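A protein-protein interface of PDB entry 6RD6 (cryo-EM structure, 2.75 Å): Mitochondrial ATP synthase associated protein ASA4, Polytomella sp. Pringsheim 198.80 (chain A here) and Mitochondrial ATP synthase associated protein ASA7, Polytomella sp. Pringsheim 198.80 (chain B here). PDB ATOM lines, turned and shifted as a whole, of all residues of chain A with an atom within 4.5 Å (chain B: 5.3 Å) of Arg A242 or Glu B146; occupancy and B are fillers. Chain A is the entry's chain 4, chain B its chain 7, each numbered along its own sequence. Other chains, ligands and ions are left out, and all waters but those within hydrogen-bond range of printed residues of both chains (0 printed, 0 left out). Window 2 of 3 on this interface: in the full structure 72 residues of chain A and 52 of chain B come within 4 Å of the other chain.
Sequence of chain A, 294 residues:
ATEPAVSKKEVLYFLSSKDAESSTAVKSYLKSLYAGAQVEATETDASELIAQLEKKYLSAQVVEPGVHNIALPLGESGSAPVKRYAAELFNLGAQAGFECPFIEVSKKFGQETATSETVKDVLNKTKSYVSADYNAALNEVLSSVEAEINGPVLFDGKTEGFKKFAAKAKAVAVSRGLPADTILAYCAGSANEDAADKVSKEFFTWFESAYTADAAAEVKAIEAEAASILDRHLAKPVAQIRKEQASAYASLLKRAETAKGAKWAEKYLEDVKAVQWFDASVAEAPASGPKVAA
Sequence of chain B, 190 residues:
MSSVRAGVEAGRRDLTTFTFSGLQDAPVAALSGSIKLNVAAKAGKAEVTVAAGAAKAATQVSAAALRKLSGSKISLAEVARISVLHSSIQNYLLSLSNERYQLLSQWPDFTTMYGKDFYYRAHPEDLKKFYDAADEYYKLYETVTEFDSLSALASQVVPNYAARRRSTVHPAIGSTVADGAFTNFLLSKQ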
ATOM      1  N   VAL A 238      32.850   0.737 -11.841  1.00  0.00           N
ATOM      2  CA  VAL A 238      32.647  -0.658 -11.465  1.00  0.00           C
ATOM      3  C   VAL A 238      33.716  -1.133 -10.491  1.00  0.00           C
ATOM      4  O   VAL A 238      33.415  -1.852  -9.531  1.00  0.00           O
ATOM      5  CB  VAL A 238      32.623  -1.545 -12.719  1.00  0.00           C
ATOM      6  CG1 VAL A 238      32.243  -2.960 -12.369  1.00  0.00           C
ATOM      7  CG2 VAL A 238      31.674  -0.975 -13.715  1.00  0.00           C
ATOM      8  N   ALA A 239      34.969  -0.738 -10.732  1.00  0.00           N
ATOM      9  CA  ALA A 239      36.080  -1.255  -9.938  1.00  0.00           C
ATOM     10  C   ALA A 239      36.048  -0.718  -8.514  1.00  0.00           C
ATOM     11  O   ALA A 239      36.413  -1.429  -7.567  1.00  0.00           O
ATOM     12  CB  ALA A 239      37.405  -0.910 -10.611  1.00  0.00           C
ATOM     13  N   GLN A 240      35.613   0.535  -8.346  1.00  0.00           N
ATOM     14  CA  GLN A 240      35.421   1.096  -7.013  1.00  0.00           C
ATOM     15  C   GLN A 240      34.336   0.347  -6.255  1.00  0.00           C
ATOM     16  O   GLN A 240      34.484   0.069  -5.059  1.00  0.00           O
ATOM     17  CB  GLN A 240      35.069   2.579  -7.121  1.00  0.00           C
ATOM     18  CG  GLN A 240      34.838   3.263  -5.793  1.00  0.00           C
ATOM     19  CD  GLN A 240      34.143   4.596  -5.939  1.00  0.00           C
ATOM     20  OE1 GLN A 240      33.518   5.089  -5.004  1.00  0.00           O
ATOM     21  NE2 GLN A 240      34.252   5.193  -7.116  1.00  0.00           N
ATOM     22  N   ILE A 241      33.261  -0.022  -6.957  1.00  0.00           N
ATOM     23  CA  ILE A 241      32.167  -0.792  -6.368  1.00  0.00           C
ATOM     24  C   ILE A 241      32.659  -2.160  -5.916  1.00  0.00           C
ATOM     25  O   ILE A 241      32.371  -2.606  -4.797  1.00  0.00           O
ATOM     26  CB  ILE A 241      31.016  -0.915  -7.382  1.00  0.00           C
ATOM     27  CG1 ILE A 241      30.254   0.396  -7.497  1.00  0.00           C
ATOM     28  CG2 ILE A 241      30.077  -2.028  -7.020  1.00  0.00           C
ATOM     29  CD1 ILE A 241      29.403   0.455  -8.715  1.00  0.00           C
ATOM     30  N   ARG A 242      33.441  -2.823  -6.773  1.00  0.00           N
ATOM     31  CA  ARG A 242      33.938  -4.161  -6.474  1.00  0.00           C
ATOM     32  C   ARG A 242      34.897  -4.148  -5.292  1.00  0.00           C
ATOM     33  O   ARG A 242      34.795  -4.993  -4.395  1.00  0.00           O
ATOM     34  CB  ARG A 242      34.621  -4.752  -7.704  1.00  0.00           C
ATOM     35  CG  ARG A 242      33.691  -5.091  -8.843  1.00  0.00           C
ATOM     36  CD  ARG A 242      34.223  -6.278  -9.616  1.00  0.00           C
ATOM     37  NE  ARG A 242      33.466  -6.535 -10.835  1.00  0.00           N
ATOM     38  CZ  ARG A 242      33.832  -6.109 -12.037  1.00  0.00           C
ATOM     39  NH1 ARG A 242      34.943  -5.401 -12.179  1.00  0.00           N
ATOM     40  NH2 ARG A 242      33.086  -6.385 -13.096  1.00  0.00           N
ATOM     41  N   LYS A 243      35.809  -3.171  -5.247  1.00  0.00           N
ATOM     42  CA  LYS A 243      36.763  -3.141  -4.141  1.00  0.00           C
ATOM     43  C   LYS A 243      36.099  -2.691  -2.841  1.00  0.00           C
ATOM     44  O   LYS A 243      36.454  -3.188  -1.767  1.00  0.00           O
ATOM     45  CB  LYS A 243      37.973  -2.267  -4.488  1.00  0.00           C
ATOM     46  CG  LYS A 243      37.724  -0.776  -4.635  1.00  0.00           C
ATOM     47  CD  LYS A 243      39.027   0.003  -4.579  1.00  0.00           C
ATOM     48  CE  LYS A 243      38.928   1.316  -5.341  1.00  0.00           C
ATOM     49  NZ  LYS A 243      39.162   1.139  -6.801  1.00  0.00           N
ATOM     50  N   GLU A 244      35.085  -1.818  -2.922  1.00  0.00           N
ATOM     51  CA  GLU A 244      34.366  -1.397  -1.723  1.00  0.00           C
ATOM     52  C   GLU A 244      33.560  -2.542  -1.129  1.00  0.00           C
ATOM     53  O   GLU A 244      33.594  -2.771   0.087  1.00  0.00           O
ATOM     54  CB  GLU A 244      33.445  -0.224  -2.049  1.00  0.00           C
ATOM     55  CG  GLU A 244      34.088   1.139  -1.925  1.00  0.00           C
ATOM     56  CD  GLU A 244      33.233   2.232  -2.531  1.00  0.00           C
ATOM     57  OE1 GLU A 244      32.127   1.917  -3.018  1.00  0.00           O
ATOM     58  OE2 GLU A 244      33.666   3.403  -2.526  1.00  0.00           O
ATOM     59  N   GLN A 245      32.850  -3.289  -1.972  1.00  0.00           N
ATOM     60  CA  GLN A 245      32.057  -4.400  -1.470  1.00  0.00           C
ATOM     61  C   GLN A 245      32.920  -5.573  -1.029  1.00  0.00           C
ATOM     62  O   GLN A 245      32.567  -6.253  -0.061  1.00  0.00           O
ATOM     63  CB  GLN A 245      31.055  -4.835  -2.530  1.00  0.00           C
ATOM     64  CG  GLN A 245      30.001  -3.790  -2.780  1.00  0.00           C
ATOM     65  CD  GLN A 245      28.977  -4.241  -3.775  1.00  0.00           C
ATOM     66  OE1 GLN A 245      29.159  -5.252  -4.447  1.00  0.00           O
ATOM     67  NE2 GLN A 245      27.885  -3.501  -3.875  1.00  0.00           N
ATOM     68  N   ALA A 246      34.062  -5.799  -1.686  1.00  0.00           N
ATOM     69  CA  ALA A 246      34.984  -6.835  -1.235  1.00  0.00           C
ATOM     70  C   ALA A 246      35.612  -6.465   0.102  1.00  0.00           C
ATOM     71  O   ALA A 246      35.797  -7.327   0.966  1.00  0.00           O
ATOM     72  CB  ALA A 246      36.061  -7.070  -2.292  1.00  0.00           C
ATOM     73  N   GLU B 142      28.492  -0.122 -17.876  1.00  0.00           N
ATOM     74  CA  GLU B 142      29.176  -1.178 -17.145  1.00  0.00           C
ATOM     75  C   GLU B 142      28.765  -1.189 -15.683  1.00  0.00           C
ATOM     76  O   GLU B 142      28.797  -2.240 -15.033  1.00  0.00           O
ATOM     77  CB  GLU B 142      30.686  -1.024 -17.286  1.00  0.00           C
ATOM     78  CG  GLU B 142      31.230  -1.605 -18.572  1.00  0.00           C
ATOM     79  CD  GLU B 142      32.715  -1.372 -18.741  1.00  0.00           C
ATOM     80  OE1 GLU B 142      33.319  -0.715 -17.866  1.00  0.00           O
ATOM     81  OE2 GLU B 142      33.277  -1.846 -19.751  1.00  0.00           O
ATOM     82  N   THR B 143      28.381  -0.033 -15.133  1.00  0.00           N
ATOM     83  CA  THR B 143      27.997  -0.034 -13.726  1.00  0.00           C
ATOM     84  C   THR B 143      26.518  -0.356 -13.543  1.00  0.00           C
ATOM     85  O   THR B 143      26.102  -0.736 -12.445  1.00  0.00           O
ATOM     86  CB  THR B 143      28.352   1.293 -13.052  1.00  0.00           C
ATOM     87  OG1 THR B 143      28.145   1.165 -11.646  1.00  0.00           O
ATOM     88  CG2 THR B 143      27.482   2.417 -13.536  1.00  0.00           C
ATOM     89  N   VAL B 144      25.702  -0.228 -14.594  1.00  0.00           N
ATOM     90  CA  VAL B 144      24.301  -0.593 -14.416  1.00  0.00           C
ATOM     91  C   VAL B 144      24.105  -2.091 -14.634  1.00  0.00           C
ATOM     92  O   VAL B 144      23.125  -2.672 -14.155  1.00  0.00           O
ATOM     93  CB  VAL B 144      23.389   0.250 -15.329  1.00  0.00           C
ATOM     94  CG1 VAL B 144      23.413  -0.250 -16.765  1.00  0.00           C
ATOM     95  CG2 VAL B 144      21.974   0.325 -14.777  1.00  0.00           C
ATOM     96  N   THR B 145      25.034  -2.750 -15.320  1.00  0.00           N
ATOM     97  CA  THR B 145      24.942  -4.181 -15.556  1.00  0.00           C
ATOM     98  C   THR B 145      25.713  -4.988 -14.529  1.00  0.00           C
ATOM     99  O   THR B 145      25.848  -6.202 -14.685  1.00  0.00           O
ATOM    100  CB  THR B 145      25.440  -4.528 -16.962  1.00  0.00           C
ATOM    101  OG1 THR B 145      26.738  -3.965 -17.162  1.00  0.00           O
ATOM    102  CG2 THR B 145      24.500  -3.977 -18.009  1.00  0.00           C
ATOM    103  N   GLU B 146      26.230  -4.340 -13.489  1.00  0.00           N
ATOM    104  CA  GLU B 146      26.877  -5.034 -12.380  1.00  0.00           C
ATOM    105  C   GLU B 146      25.797  -5.459 -11.383  1.00  0.00           C
ATOM    106  O   GLU B 146      25.605  -4.868 -10.320  1.00  0.00           O
ATOM    107  CB  GLU B 146      27.930  -4.139 -11.745  1.00  0.00           C
ATOM    108  CG  GLU B 146      28.916  -4.850 -10.850  1.00  0.00           C
ATOM    109  CD  GLU B 146      29.697  -5.923 -11.564  1.00  0.00           C
ATOM    110  OE1 GLU B 146      30.215  -5.650 -12.665  1.00  0.00           O
ATOM    111  OE2 GLU B 146      29.801  -7.040 -11.020  1.00  0.00           O
ATOM    112  N   PHE B 147      25.069  -6.513 -11.763  1.00  0.00           N
ATOM    113  CA  PHE B 147      23.923  -6.952 -10.976  1.00  0.00           C
ATOM    114  C   PHE B 147      24.347  -7.696  -9.719  1.00  0.00           C
ATOM    115  O   PHE B 147      23.604  -7.707  -8.730  1.00  0.00           O
ATOM    116  CB  PHE B 147      23.013  -7.834 -11.819  1.00  0.00           C
ATOM    117  CG  PHE B 147      22.507  -7.170 -13.059  1.00  0.00           C
ATOM    118  CD1 PHE B 147      21.702  -6.051 -12.980  1.00  0.00           C
ATOM    119  CD2 PHE B 147      22.835  -7.670 -14.307  1.00  0.00           C
ATOM    120  CE1 PHE B 147      21.233  -5.442 -14.121  1.00  0.00           C
ATOM    121  CE2 PHE B 147      22.368  -7.063 -15.448  1.00  0.00           C
ATOM    122  CZ  PHE B 147      21.563  -5.952 -15.356  1.00  0.00           C
ATOM    123  N   ASP B 148      25.545  -8.289  -9.725  1.00  0.00           N
ATOM    124  CA  ASP B 148      26.027  -9.043  -8.569  1.00  0.00           C
ATOM    125  C   ASP B 148      26.312  -8.135  -7.380  1.00  0.00           C
ATOM    126  O   ASP B 148      26.423  -8.606  -6.243  1.00  0.00           O
ATOM    127  CB  ASP B 148      27.281  -9.827  -8.942  1.00  0.00           C
ATOM    128  CG  ASP B 148      27.005 -10.923  -9.938  1.00  0.00           C
ATOM    129  OD1 ASP B 148      25.838 -11.065 -10.356  1.00  0.00           O
ATOM    130  OD2 ASP B 148      27.955 -11.644 -10.303  1.00  0.00           O
ATOM    131  N   SER B 149      26.445  -6.832  -7.624  1.00  0.00           N
ATOM    132  CA  SER B 149      26.609  -5.883  -6.537  1.00  0.00           C
ATOM    133  C   SER B 149      25.303  -5.631  -5.804  1.00  0.00           C
ATOM    134  O   SER B 149      25.328  -5.245  -4.628  1.00  0.00           O
ATOM    135  CB  SER B 149      27.165  -4.577  -7.082  1.00  0.00           C
ATOM    136  OG  SER B 149      28.445  -4.795  -7.629  1.00  0.00           O
ATOM    137  N   LEU B 150      24.166  -5.875  -6.473  1.00  0.00           N
ATOM    138  CA  LEU B 150      22.861  -5.444  -5.972  1.00  0.00           C
ATOM    139  C   LEU B 150      22.505  -6.119  -4.657  1.00  0.00           C
ATOM    140  O   LEU B 150      21.925  -5.482  -3.768  1.00  0.00           O
ATOM    141  CB  LEU B 150      21.780  -5.730  -7.012  1.00  0.00           C
ATOM    142  CG  LEU B 150      21.736  -4.849  -8.250  1.00  0.00           C
ATOM    143  CD1 LEU B 150      20.551  -5.225  -9.105  1.00  0.00           C
ATOM    144  CD2 LEU B 150      21.666  -3.403  -7.848  1.00  0.00           C
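The side-chain carboxylate of Glu B146 lies within salt-bridge range of the guanidinium group of Arg A242 (3.0 Å).
The backbone carbonyl oxygen of Ser B149 is in hydrogen-bond range of the side-chain amide nitrogen of Gln A245 (3.2 Å).
The side-chain hydroxyl (OG1) of Thr B145 lies within hydrogen-bond range of the backbone carbonyl oxygen (O) of Glu B142.
Among the printed residues, merely in contact across the chains: Ile A241 with Thr B143, Ile A241 with Ser B149, Val A238 with Glu B146, Val A238 with Glu B142 and Val A238 with Thr B143.
Arg A242 touches just one residue of chain B: Glu B146 (3.0 Å).
Printed residues of chain A within 4 Å of Glu B146: Val A238 (3.4 Å) and Arg A242 (3.0 Å).
Printed residues of chain A within 4 Å of Thr B143: Val A238 (3.7 Å) and Ile A241 (3.3 Å).
Of the printed residues of chain B, Val A238 touches Glu B142, Thr B143 and Glu B146.
Of the printed residues of chain A, Ser B149 touches Ile A241 and Gln A245.
Printed residues of chain A within 4 Å of Glu B142: Val A238 (3.4 Å).
Phe B147 touches none of the printed residues of chain A.
The nearest printed residue of chain A that does not touch Glu B146 is Ile A241 (4.9 Å).
The nearest printed residue of chain A that does not touch Thr B143 is Ala A239 (7.1 Å).
Of the 9 printed residues of chain A, 4 touch a printed residue of chain B.
Printed residues of chain A that touch a printed residue of chain B: Val A238, Ile A241, Arg A242 and Gln A245.
Hydrophobic or aromatic side chains of chain A that line the printed part of chain B: Val A238 and Ile A241.
Of the 9 printed residues of chain B, 4 touch a printed residue of chain A.
Among the printed residues, Asp or Glu carboxylates within 4 Å of a Lys or Arg side-chain nitrogen of the other chain: Arg A242 with Glu B146 (3.0 Å).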
